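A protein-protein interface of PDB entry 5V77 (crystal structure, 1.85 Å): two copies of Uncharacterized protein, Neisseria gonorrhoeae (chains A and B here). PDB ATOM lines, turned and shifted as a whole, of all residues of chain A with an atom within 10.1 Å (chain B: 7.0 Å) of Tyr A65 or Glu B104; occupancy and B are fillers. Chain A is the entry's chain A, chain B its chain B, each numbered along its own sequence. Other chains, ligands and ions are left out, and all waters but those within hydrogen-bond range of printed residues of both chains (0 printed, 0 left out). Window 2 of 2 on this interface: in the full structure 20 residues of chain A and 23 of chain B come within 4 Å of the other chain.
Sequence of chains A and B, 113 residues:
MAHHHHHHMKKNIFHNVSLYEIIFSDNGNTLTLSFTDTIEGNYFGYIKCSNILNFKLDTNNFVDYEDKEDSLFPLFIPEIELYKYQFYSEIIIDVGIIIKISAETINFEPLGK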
ATOM      1  N   LEU A  57      12.156 -26.127  29.803  1.00  0.00           N
ATOM      2  CA  LEU A  57      13.398 -26.435  30.490  1.00  0.00           C
ATOM      3  C   LEU A  57      14.501 -25.685  29.766  1.00  0.00           C
ATOM      4  O   LEU A  57      14.680 -25.861  28.562  1.00  0.00           O
ATOM      5  CB  LEU A  57      13.683 -27.941  30.488  1.00  0.00           C
ATOM      6  CG  LEU A  57      15.132 -28.338  30.815  1.00  0.00           C
ATOM      7  CD1 LEU A  57      15.442 -28.070  32.252  1.00  0.00           C
ATOM      8  CD2 LEU A  57      15.381 -29.797  30.486  1.00  0.00           C
ATOM      9  N   ASP A  58      15.235 -24.847  30.488  1.00  0.00           N
ATOM     10  CA  ASP A  58      16.351 -24.123  29.898  1.00  0.00           C
ATOM     11  C   ASP A  58      17.552 -24.345  30.800  1.00  0.00           C
ATOM     12  O   ASP A  58      17.512 -23.975  31.979  1.00  0.00           O
ATOM     13  CB  ASP A  58      16.023 -22.637  29.751  1.00  0.00           C
ATOM     14  CG  ASP A  58      17.148 -21.842  29.114  1.00  0.00           C
ATOM     15  OD1 ASP A  58      18.212 -22.414  28.780  1.00  0.00           O
ATOM     16  OD2 ASP A  58      16.962 -20.621  28.956  1.00  0.00           O
ATOM     17  N   THR A  59      18.615 -24.955  30.257  1.00  0.00           N
ATOM     18  CA  THR A  59      19.764 -25.242  31.111  1.00  0.00           C
ATOM     19  C   THR A  59      20.616 -24.008  31.364  1.00  0.00           C
ATOM     20  O   THR A  59      21.443 -24.027  32.279  1.00  0.00           O
ATOM     21  CB  THR A  59      20.613 -26.375  30.528  1.00  0.00           C
ATOM     22  OG1 THR A  59      20.993 -26.065  29.187  1.00  0.00           O
ATOM     23  CG2 THR A  59      19.815 -27.668  30.540  1.00  0.00           C
ATOM     24  N   ASN A  60      20.430 -22.946  30.580  1.00  0.00           N
ATOM     25  CA  ASN A  60      21.018 -21.638  30.876  1.00  0.00           C
ATOM     26  C   ASN A  60      22.535 -21.709  31.034  1.00  0.00           C
ATOM     27  O   ASN A  60      23.111 -21.057  31.906  1.00  0.00           O
ATOM     28  CB  ASN A  60      20.383 -21.030  32.127  1.00  0.00           C
ATOM     29  CG  ASN A  60      19.565 -19.801  31.822  1.00  0.00           C
ATOM     30  OD1 ASN A  60      18.410 -19.899  31.405  1.00  0.00           O
ATOM     31  ND2 ASN A  60      20.157 -18.630  32.031  1.00  0.00           N
ATOM     32  N   ASN A  61      23.185 -22.508  30.186  1.00  0.00           N
ATOM     33  CA  ASN A  61      24.646 -22.648  30.209  1.00  0.00           C
ATOM     34  C   ASN A  61      25.148 -22.946  31.620  1.00  0.00           C
ATOM     35  O   ASN A  61      26.243 -22.536  32.005  1.00  0.00           O
ATOM     36  CB  ASN A  61      25.336 -21.399  29.642  1.00  0.00           C
ATOM     37  CG  ASN A  61      26.744 -21.684  29.133  1.00  0.00           C
ATOM     38  OD1 ASN A  61      27.084 -22.826  28.821  1.00  0.00           O
ATOM     39  ND2 ASN A  61      27.571 -20.643  29.052  1.00  0.00           N
ATOM     40  N   PHE A  62      24.334 -23.653  32.403  1.00  0.00           N
ATOM     41  CA  PHE A  62      24.677 -23.995  33.775  1.00  0.00           C
ATOM     42  C   PHE A  62      25.362 -25.349  33.880  1.00  0.00           C
ATOM     43  O   PHE A  62      26.328 -25.494  34.640  1.00  0.00           O
ATOM     44  CB  PHE A  62      23.425 -23.983  34.655  1.00  0.00           C
ATOM     45  CG  PHE A  62      23.702 -24.292  36.096  1.00  0.00           C
ATOM     46  CD1 PHE A  62      23.712 -25.602  36.548  1.00  0.00           C
ATOM     47  CD2 PHE A  62      23.951 -23.271  37.003  1.00  0.00           C
ATOM     48  CE1 PHE A  62      23.975 -25.891  37.872  1.00  0.00           C
ATOM     49  CE2 PHE A  62      24.207 -23.555  38.335  1.00  0.00           C
ATOM     50  CZ  PHE A  62      24.219 -24.865  38.772  1.00  0.00           C
ATOM     51  N   VAL A  63      24.867 -26.350  33.158  1.00  0.00           N
ATOM     52  CA  VAL A  63      25.488 -27.669  33.154  1.00  0.00           C
ATOM     53  C   VAL A  63      26.743 -27.611  32.298  1.00  0.00           C
ATOM     54  O   VAL A  63      26.708 -27.146  31.153  1.00  0.00           O
ATOM     55  CB  VAL A  63      24.513 -28.737  32.631  1.00  0.00           C
ATOM     56  CG1 VAL A  63      25.092 -30.129  32.838  1.00  0.00           C
ATOM     57  CG2 VAL A  63      23.168 -28.616  33.318  1.00  0.00           C
ATOM     58  N   ASP A  64      27.861 -28.067  32.859  1.00  0.00           N
ATOM     59  CA  ASP A  64      29.103 -28.201  32.107  1.00  0.00           C
ATOM     60  C   ASP A  64      29.093 -29.582  31.471  1.00  0.00           C
ATOM     61  O   ASP A  64      29.328 -30.589  32.143  1.00  0.00           O
ATOM     62  CB  ASP A  64      30.318 -28.010  33.008  1.00  0.00           C
ATOM     63  CG  ASP A  64      31.623 -28.097  32.244  1.00  0.00           C
ATOM     64  OD1 ASP A  64      31.587 -28.093  30.994  1.00  0.00           O
ATOM     65  OD2 ASP A  64      32.689 -28.173  32.892  1.00  0.00           O
ATOM     66  N   TYR A  65      28.812 -29.634  30.171  1.00  0.00           N
ATOM     67  CA  TYR A  65      28.762 -30.914  29.482  1.00  0.00           C
ATOM     68  C   TYR A  65      30.147 -31.479  29.199  1.00  0.00           C
ATOM     69  O   TYR A  65      30.279 -32.693  29.017  1.00  0.00           O
ATOM     70  CB  TYR A  65      27.949 -30.774  28.195  1.00  0.00           C
ATOM     71  CG  TYR A  65      26.482 -30.563  28.482  1.00  0.00           C
ATOM     72  CD1 TYR A  65      25.756 -31.525  29.172  1.00  0.00           C
ATOM     73  CD2 TYR A  65      25.822 -29.403  28.087  1.00  0.00           C
ATOM     74  CE1 TYR A  65      24.415 -31.356  29.454  1.00  0.00           C
ATOM     75  CE2 TYR A  65      24.462 -29.223  28.366  1.00  0.00           C
ATOM     76  CZ  TYR A  65      23.772 -30.208  29.051  1.00  0.00           C
ATOM     77  OH  TYR A  65      22.434 -30.064  29.347  1.00  0.00           O
ATOM     78  N   GLU A  66      31.180 -30.635  29.176  1.00  0.00           N
ATOM     79  CA  GLU A  66      32.545 -31.147  29.173  1.00  0.00           C
ATOM     80  C   GLU A  66      32.867 -31.906  30.457  1.00  0.00           C
ATOM     81  O   GLU A  66      33.777 -32.743  30.458  1.00  0.00           O
ATOM     82  CB  GLU A  66      33.533 -29.996  28.971  1.00  0.00           C
ATOM     83  N   ASP A  67      32.136 -31.638  31.544  1.00  0.00           N
ATOM     84  CA  ASP A  67      32.329 -32.329  32.816  1.00  0.00           C
ATOM     85  C   ASP A  67      31.569 -33.648  32.804  1.00  0.00           C
ATOM     86  O   ASP A  67      30.342 -33.659  32.689  1.00  0.00           O
ATOM     87  CB  ASP A  67      31.850 -31.453  33.974  1.00  0.00           C
ATOM     88  CG  ASP A  67      32.091 -32.089  35.340  1.00  0.00           C
ATOM     89  OD1 ASP A  67      32.665 -33.197  35.404  1.00  0.00           O
ATOM     90  OD2 ASP A  67      31.705 -31.474  36.357  1.00  0.00           O
ATOM     91  N   LYS A  68      32.294 -34.758  32.952  1.00  0.00           N
ATOM     92  CA  LYS A  68      31.647 -36.067  32.941  1.00  0.00           C
ATOM     93  C   LYS A  68      30.679 -36.222  34.109  1.00  0.00           C
ATOM     94  O   LYS A  68      29.611 -36.826  33.964  1.00  0.00           O
ATOM     95  CB  LYS A  68      32.704 -37.172  32.971  1.00  0.00           C
ATOM     96  N   GLU A  69      31.027 -35.676  35.271  1.00  0.00           N
ATOM     97  CA  GLU A  69      30.236 -35.898  36.476  1.00  0.00           C
ATOM     98  C   GLU A  69      29.037 -34.967  36.593  1.00  0.00           C
ATOM     99  O   GLU A  69      28.315 -35.043  37.594  1.00  0.00           O
ATOM    100  CB  GLU A  69      31.121 -35.749  37.717  1.00  0.00           C
ATOM    101  N   ASP A  70      28.790 -34.108  35.609  1.00  0.00           N
ATOM    102  CA  ASP A  70      27.759 -33.087  35.729  1.00  0.00           C
ATOM    103  C   ASP A  70      26.530 -33.480  34.918  1.00  0.00           C
ATOM    104  O   ASP A  70      26.645 -33.869  33.751  1.00  0.00           O
ATOM    105  CB  ASP A  70      28.279 -31.724  35.275  1.00  0.00           C
ATOM    106  CG  ASP A  70      27.443 -30.579  35.817  1.00  0.00           C
ATOM    107  OD1 ASP A  70      26.390 -30.851  36.439  1.00  0.00           O
ATOM    108  OD2 ASP A  70      27.841 -29.413  35.627  1.00  0.00           O
ATOM    109  N   SER A  71      25.361 -33.371  35.536  1.00  0.00           N
ATOM    110  CA  SER A  71      24.143 -33.767  34.844  1.00  0.00           C
ATOM    111  C   SER A  71      22.950 -33.066  35.477  1.00  0.00           C
ATOM    112  O   SER A  71      23.032 -32.520  36.579  1.00  0.00           O
ATOM    113  CB  SER A  71      23.961 -35.284  34.869  1.00  0.00           C
ATOM    114  OG  SER A  71      23.667 -35.728  36.176  1.00  0.00           O
ATOM    115  N   LEU A  72      21.838 -33.085  34.746  1.00  0.00           N
ATOM    116  CA  LEU A  72      20.638 -32.393  35.202  1.00  0.00           C
ATOM    117  C   LEU A  72      20.114 -33.001  36.498  1.00  0.00           C
ATOM    118  O   LEU A  72      19.900 -32.291  37.484  1.00  0.00           O
ATOM    119  CB  LEU A  72      19.579 -32.436  34.108  1.00  0.00           C
ATOM    120  CG  LEU A  72      18.182 -31.919  34.452  1.00  0.00           C
ATOM    121  CD1 LEU A  72      18.240 -30.441  34.800  1.00  0.00           C
ATOM    122  CD2 LEU A  72      17.227 -32.183  33.271  1.00  0.00           C
ATOM    123  N   PHE A  73      19.902 -34.315  36.514  1.00  0.00           N
ATOM    124  CA  PHE A  73      19.422 -35.076  37.663  1.00  0.00           C
ATOM    125  C   PHE A  73      20.590 -35.727  38.391  1.00  0.00           C
ATOM    126  O   PHE A  73      21.511 -36.229  37.748  1.00  0.00           O
ATOM    127  CB  PHE A  73      18.448 -36.174  37.235  1.00  0.00           C
ATOM    128  CG  PHE A  73      17.247 -35.675  36.484  1.00  0.00           C
ATOM    129  CD1 PHE A  73      16.599 -34.503  36.850  1.00  0.00           C
ATOM    130  CD2 PHE A  73      16.758 -36.397  35.409  1.00  0.00           C
ATOM    131  CE1 PHE A  73      15.472 -34.059  36.144  1.00  0.00           C
ATOM    132  CE2 PHE A  73      15.636 -35.964  34.697  1.00  0.00           C
ATOM    133  CZ  PHE A  73      15.003 -34.796  35.050  1.00  0.00           C
ATOM    134  N   ILE A  97      19.672 -23.703  36.173  1.00  0.00           N
ATOM    135  CA  ILE A  97      18.696 -24.314  35.286  1.00  0.00           C
ATOM    136  C   ILE A  97      17.319 -23.784  35.664  1.00  0.00           C
ATOM    137  O   ILE A  97      17.026 -23.563  36.844  1.00  0.00           O
ATOM    138  CB  ILE A  97      18.793 -25.843  35.413  1.00  0.00           C
ATOM    139  CG1 ILE A  97      20.129 -26.319  34.832  1.00  0.00           C
ATOM    140  CG2 ILE A  97      17.610 -26.535  34.780  1.00  0.00           C
ATOM    141  CD1 ILE A  97      20.727 -27.467  35.582  1.00  0.00           C
ATOM    142  N   GLY B  28      19.268 -37.214  33.049  1.00  0.00           N
ATOM    143  CA  GLY B  28      18.565 -36.069  32.510  1.00  0.00           C
ATOM    144  C   GLY B  28      19.282 -35.328  31.405  1.00  0.00           C
ATOM    145  O   GLY B  28      18.753 -34.322  30.916  1.00  0.00           O
ATOM    146  N   ASN B  29      20.468 -35.782  31.004  1.00  0.00           N
ATOM    147  CA  ASN B  29      21.232 -35.107  29.967  1.00  0.00           C
ATOM    148  C   ASN B  29      20.737 -35.417  28.568  1.00  0.00           C
ATOM    149  O   ASN B  29      21.117 -34.705  27.631  1.00  0.00           O
ATOM    150  CB  ASN B  29      22.704 -35.486  30.054  1.00  0.00           C
ATOM    151  CG  ASN B  29      23.394 -34.859  31.240  1.00  0.00           C
ATOM    152  OD1 ASN B  29      22.795 -34.058  31.970  1.00  0.00           O
ATOM    153  ND2 ASN B  29      24.663 -35.203  31.440  1.00  0.00           N
ATOM    154  N   THR B  30      19.926 -36.456  28.401  1.00  0.00           N
ATOM    155  CA  THR B  30      19.459 -36.901  27.094  1.00  0.00           C
ATOM    156  C   THR B  30      17.943 -36.981  27.084  1.00  0.00           C
ATOM    157  O   THR B  30      17.324 -37.388  28.071  1.00  0.00           O
ATOM    158  CB  THR B  30      20.046 -38.267  26.743  1.00  0.00           C
ATOM    159  OG1 THR B  30      21.472 -38.165  26.725  1.00  0.00           O
ATOM    160  CG2 THR B  30      19.577 -38.724  25.385  1.00  0.00           C
ATOM    161  N   CYS B  49      18.275 -36.516  21.662  1.00  0.00           N
ATOM    162  CA  CYS B  49      18.869 -35.201  21.852  1.00  0.00           C
ATOM    163  C   CYS B  49      19.810 -35.285  23.047  1.00  0.00           C
ATOM    164  O   CYS B  49      19.362 -35.554  24.161  1.00  0.00           O
ATOM    165  CB  CYS B  49      17.771 -34.157  22.081  1.00  0.00           C
ATOM    166  SG  CYS B  49      16.495 -34.131  20.742  1.00  0.00           S
ATOM    167  N   SER B  50      21.110 -35.098  22.814  1.00  0.00           N
ATOM    168  CA  SER B  50      22.113 -35.285  23.854  1.00  0.00           C
ATOM    169  C   SER B  50      22.670 -33.939  24.291  1.00  0.00           C
ATOM    170  O   SER B  50      22.936 -33.069  23.457  1.00  0.00           O
ATOM    171  CB  SER B  50      23.256 -36.188  23.367  1.00  0.00           C
ATOM    172  OG  SER B  50      22.751 -37.424  22.876  1.00  0.00           O
ATOM    173  N   ASN B  51      22.856 -33.785  25.603  1.00  0.00           N
ATOM    174  CA  ASN B  51      23.278 -32.522  26.198  1.00  0.00           C
ATOM    175  C   ASN B  51      22.300 -31.408  25.861  1.00  0.00           C
ATOM    176  O   ASN B  51      22.576 -30.538  25.023  1.00  0.00           O
ATOM    177  CB  ASN B  51      24.691 -32.171  25.753  1.00  0.00           C
ATOM    178  CG  ASN B  51      25.696 -33.180  26.246  1.00  0.00           C
ATOM    179  OD1 ASN B  51      25.357 -34.060  27.040  1.00  0.00           O
ATOM    180  ND2 ASN B  51      26.935 -33.063  25.789  1.00  0.00           N
ATOM    181  N   ILE B  52      21.171 -31.421  26.568  1.00  0.00           N
ATOM    182  CA  ILE B  52      20.054 -30.540  26.274  1.00  0.00           C
ATOM    183  C   ILE B  52      20.427 -29.106  26.598  1.00  0.00           C
ATOM    184  O   ILE B  52      21.051 -28.817  27.628  1.00  0.00           O
ATOM    185  CB  ILE B  52      18.812 -30.964  27.076  1.00  0.00           C
ATOM    186  CG1 ILE B  52      18.455 -32.418  26.777  1.00  0.00           C
ATOM    187  CG2 ILE B  52      17.649 -30.046  26.768  1.00  0.00           C
ATOM    188  CD1 ILE B  52      18.107 -32.662  25.334  1.00  0.00           C
ATOM    189  N   LEU B  53      20.039 -28.196  25.712  1.00  0.00           N
ATOM    190  CA  LEU B  53      20.154 -26.765  25.955  1.00  0.00           C
ATOM    191  C   LEU B  53      18.805 -26.172  26.338  1.00  0.00           C
ATOM    192  O   LEU B  53      18.688 -25.504  27.369  1.00  0.00           O
ATOM    193  CB  LEU B  53      20.727 -26.065  24.712  1.00  0.00           C
ATOM    194  CG  LEU B  53      22.082 -26.600  24.255  1.00  0.00           C
ATOM    195  CD1 LEU B  53      22.462 -25.996  22.908  1.00  0.00           C
ATOM    196  CD2 LEU B  53      23.170 -26.324  25.294  1.00  0.00           C
ATOM    197  N   LYS B  84      20.778 -27.915  11.818  1.00  0.00           N
ATOM    198  CA  LYS B  84      22.110 -28.241  12.314  1.00  0.00           C
ATOM    199  C   LYS B  84      22.945 -26.971  12.241  1.00  0.00           C
ATOM    200  O   LYS B  84      23.383 -26.570  11.162  1.00  0.00           O
ATOM    201  CB  LYS B  84      22.740 -29.380  11.518  1.00  0.00           C
ATOM    202  CG  LYS B  84      24.169 -29.709  11.955  1.00  0.00           C
ATOM    203  CD  LYS B  84      24.377 -31.208  12.165  1.00  0.00           C
ATOM    204  CE  LYS B  84      25.814 -31.526  12.576  1.00  0.00           C
ATOM    205  NZ  LYS B  84      26.682 -30.314  12.599  1.00  0.00           N
ATOM    206  N   TYR B  85      23.155 -26.337  13.390  1.00  0.00           N
ATOM    207  CA  TYR B  85      24.030 -25.180  13.481  1.00  0.00           C
ATOM    208  C   TYR B  85      25.461 -25.650  13.722  1.00  0.00           C
ATOM    209  O   TYR B  85      25.735 -26.842  13.883  1.00  0.00           O
ATOM    210  CB  TYR B  85      23.550 -24.234  14.584  1.00  0.00           C
ATOM    211  CG  TYR B  85      22.125 -23.768  14.376  1.00  0.00           C
ATOM    212  CD1 TYR B  85      21.822 -22.820  13.409  1.00  0.00           C
ATOM    213  CD2 TYR B  85      21.081 -24.287  15.133  1.00  0.00           C
ATOM    214  CE1 TYR B  85      20.523 -22.392  13.205  1.00  0.00           C
ATOM    215  CE2 TYR B  85      19.775 -23.866  14.935  1.00  0.00           C
ATOM    216  CZ  TYR B  85      19.507 -22.918  13.967  1.00  0.00           C
ATOM    217  OH  TYR B  85      18.221 -22.487  13.758  1.00  0.00           O
ATOM    218  N   GLN B  86      26.392 -24.699  13.747  1.00  0.00           N
ATOM    219  CA  GLN B  86      27.794 -25.062  13.887  1.00  0.00           C
ATOM    220  C   GLN B  86      28.057 -25.806  15.190  1.00  0.00           C
ATOM    221  O   GLN B  86      28.804 -26.791  15.207  1.00  0.00           O
ATOM    222  CB  GLN B  86      28.662 -23.815  13.804  1.00  0.00           C
ATOM    223  CG  GLN B  86      30.134 -24.103  13.906  1.00  0.00           C
ATOM    224  CD  GLN B  86      30.945 -23.035  13.220  1.00  0.00           C
ATOM    225  OE1 GLN B  86      30.604 -21.853  13.275  1.00  0.00           O
ATOM    226  NE2 GLN B  86      32.005 -23.443  12.545  1.00  0.00           N
ATOM    227  N   PHE B  87      27.440 -25.363  16.291  1.00  0.00           N
ATOM    228  CA  PHE B  87      27.764 -25.905  17.601  1.00  0.00           C
ATOM    229  C   PHE B  87      26.611 -26.612  18.303  1.00  0.00           C
ATOM    230  O   PHE B  87      26.803 -27.072  19.434  1.00  0.00           O
ATOM    231  CB  PHE B  87      28.286 -24.797  18.524  1.00  0.00           C
ATOM    232  CG  PHE B  87      29.512 -24.109  18.012  1.00  0.00           C
ATOM    233  CD1 PHE B  87      30.722 -24.769  17.972  1.00  0.00           C
ATOM    234  CD2 PHE B  87      29.453 -22.794  17.592  1.00  0.00           C
ATOM    235  CE1 PHE B  87      31.862 -24.126  17.506  1.00  0.00           C
ATOM    236  CE2 PHE B  87      30.577 -22.149  17.144  1.00  0.00           C
ATOM    237  CZ  PHE B  87      31.782 -22.818  17.095  1.00  0.00           C
ATOM    238  N   TYR B  88      25.426 -26.685  17.700  1.00  0.00           N
ATOM    239  CA  TYR B  88      24.307 -27.419  18.290  1.00  0.00           C
ATOM    240  C   TYR B  88      23.278 -27.672  17.198  1.00  0.00           C
ATOM    241  O   TYR B  88      23.399 -27.172  16.076  1.00  0.00           O
ATOM    242  CB  TYR B  88      23.683 -26.663  19.479  1.00  0.00           C
ATOM    243  CG  TYR B  88      22.893 -25.432  19.084  1.00  0.00           C
ATOM    244  CD1 TYR B  88      23.539 -24.229  18.815  1.00  0.00           C
ATOM    245  CD2 TYR B  88      21.502 -25.473  18.970  1.00  0.00           C
ATOM    246  CE1 TYR B  88      22.832 -23.106  18.431  1.00  0.00           C
ATOM    247  CE2 TYR B  88      20.778 -24.344  18.587  1.00  0.00           C
ATOM    248  CZ  TYR B  88      21.461 -23.163  18.325  1.00  0.00           C
ATOM    249  OH  TYR B  88      20.781 -22.033  17.947  1.00  0.00           O
ATOM    250  N   SER B  89      22.259 -28.464  17.534  1.00  0.00           N
ATOM    251  CA  SER B  89      21.164 -28.739  16.614  1.00  0.00           C
ATOM    252  C   SER B  89      19.840 -28.484  17.316  1.00  0.00           C
ATOM    253  O   SER B  89      19.775 -28.390  18.546  1.00  0.00           O
ATOM    254  CB  SER B  89      21.228 -30.181  16.073  1.00  0.00           C
ATOM    255  OG  SER B  89      22.430 -30.378  15.321  1.00  0.00           O
ATOM    256  N   SER B 102      16.590 -27.886  21.570  1.00  0.00           N
ATOM    257  CA  SER B 102      17.964 -27.621  21.177  1.00  0.00           C
ATOM    258  C   SER B 102      18.916 -28.444  22.041  1.00  0.00           C
ATOM    259  O   SER B 102      18.775 -28.492  23.272  1.00  0.00           O
ATOM    260  CB  SER B 102      18.279 -26.130  21.323  1.00  0.00           C
ATOM    261  OG  SER B 102      17.434 -25.368  20.470  1.00  0.00           O
ATOM    262  N   ALA B 103      19.897 -29.069  21.401  1.00  0.00           N
ATOM    263  CA  ALA B 103      20.843 -29.919  22.112  1.00  0.00           C
ATOM    264  C   ALA B 103      22.171 -29.863  21.388  1.00  0.00           C
ATOM    265  O   ALA B 103      22.226 -29.570  20.190  1.00  0.00           O
ATOM    266  CB  ALA B 103      20.363 -31.374  22.183  1.00  0.00           C
ATOM    267  N   GLU B 104      23.244 -30.183  22.113  1.00  0.00           N
ATOM    268  CA  GLU B 104      24.557 -30.171  21.474  1.00  0.00           C
ATOM    269  C   GLU B 104      24.617 -31.159  20.312  1.00  0.00           C
ATOM    270  O   GLU B 104      25.203 -30.860  19.262  1.00  0.00           O
ATOM    271  CB  GLU B 104      25.648 -30.464  22.498  1.00  0.00           C
ATOM    272  CG  GLU B 104      25.752 -29.391  23.571  1.00  0.00           C
ATOM    273  CD  GLU B 104      27.075 -29.423  24.310  1.00  0.00           C
ATOM    274  OE1 GLU B 104      27.711 -30.501  24.356  1.00  0.00           O
ATOM    275  OE2 GLU B 104      27.473 -28.366  24.848  1.00  0.00           O
ATOM    276  N   THR B 105      24.018 -32.342  20.473  1.00  0.00           N
ATOM    277  CA  THR B 105      23.932 -33.294  19.375  1.00  0.00           C
ATOM    278  C   THR B 105      22.518 -33.848  19.284  1.00  0.00           C
ATOM    279  O   THR B 105      21.847 -34.048  20.301  1.00  0.00           O
ATOM    280  CB  THR B 105      24.937 -34.458  19.519  1.00  0.00           C
ATOM    281  OG1 THR B 105      24.533 -35.327  20.575  1.00  0.00           O
ATOM    282  CG2 THR B 105      26.330 -33.941  19.822  1.00  0.00           C
ATOM    283  N   ILE B 106      22.071 -34.084  18.054  1.00  0.00           N
ATOM    284  CA  ILE B 106      20.784 -34.715  17.799  1.00  0.00           C
ATOM    285  C   ILE B 106      21.018 -35.791  16.757  1.00  0.00           C
ATOM    286  O   ILE B 106      21.582 -35.512  15.690  1.00  0.00           O
ATOM    287  CB  ILE B 106      19.714 -33.713  17.332  1.00  0.00           C
ATOM    288  CG1 ILE B 106      19.423 -32.692  18.429  1.00  0.00           C
ATOM    289  CG2 ILE B 106      18.426 -34.443  16.952  1.00  0.00           C
ATOM    290  CD1 ILE B 106      18.322 -31.725  18.062  1.00  0.00           C
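The backbone carbonyl oxygen (O) of Ile B52 is in hydrogen-bond range of the side-chain hydroxyl (OG1) of Thr A59. The backbone carbonyl oxygen of Leu B53 is in hydrogen-bond range of the backbone NH of Thr A59 (2.9 Å). The side-chain hydroxyl (OH) of Tyr A65 lies within hydrogen-bond range of the backbone carbonyl oxygen (O) of Ile B52 (2.5 Å). The backbone carbonyl oxygen (O) of Asp A70 is in hydrogen-bond range of the side-chain amide nitrogen (ND2) of Asn B29 (3.3 Å). The backbone NH (N) of Leu A72 lies within hydrogen-bond range of the side-chain amide oxygen (OD1) of Asn B29 (3.1 Å). The side-chain carboxylate (OD1) of Asp A58 lies close to the backbone carbonyl oxygen (O) of Leu B53 (3.4 Å).
The side-chain carboxylate of Asp A58 lies within hydrogen-bond range of the backbone NH of Asn A60, 2.9 Å away. N of Asp A64 lies within hydrogen-bond range of OD2 of Asp A70, at 3.1 Å. OG of Ser A71 lies within hydrogen-bond range of O of Phe A73 (2.7 Å). The backbone NH of Asn B51 is in hydrogen-bond range of the backbone carbonyl oxygen of Asn B29 (2.8 Å). The backbone NH (N) of Ile B52 lies within hydrogen-bond range of the backbone carbonyl oxygen (O) of Asn B29. The backbone NH (N) of Glu B104 sits at hydrogen-bond distance from the backbone carbonyl oxygen (O) of Ser B50 (3.2 Å).
Among the printed residues, pairs that only touch across the chains: Ser A71 with Asn B29 (3.2 Å), Tyr A65 with Asn B51 (3.3 Å), Phe A73 with Gly B28 (3.4 Å), Leu A72 with Gly B28 (3.5 Å) and Tyr A65 with Glu B104 (3.8 Å).
Of chain B, only Asn B51 (3.3 Å), Ile B52 (2.5 Å) and Glu B104 (3.8 Å) come within 4 Å of Tyr A65. Glu A66 touches none of the printed residues of chain B. Of the printed residues of chain B, Leu A72 touches Gly B28 (3.5 Å) and Asn B29 (3.1 Å). Of the printed residues of chain A, Ile B52 touches Thr A59 and Tyr A65. Of the printed residues of chain A, Leu B53 touches Asp A58 (3.4 Å) and Thr A59 (2.9 Å). Gln B86 touches none of the printed residues of chain A. No residue of chain A comes within 4 Å of Ala B103. Of chain A, only Tyr A65 comes within 4 Å of Glu B104. No residue of chain A comes within 4 Å of Thr B105. The nearest printed residue of chain A that does not touch Ile B52 is Leu A57 (4.4 Å).
Of the 19 printed residues of chain B, 6 touch a printed residue of chain A. Of the 18 printed residues of chain A, 7 touch a printed residue of chain B. Hydrophobic or aromatic side chains of chain A within 4 Å of the printed part of chain B: Tyr A65, Leu A72 and Phe A73.
No position is printed for both chains. Of the 11 pairs that touch across the chains among the printed residues, none has its exchanged pair printed and touching as well.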
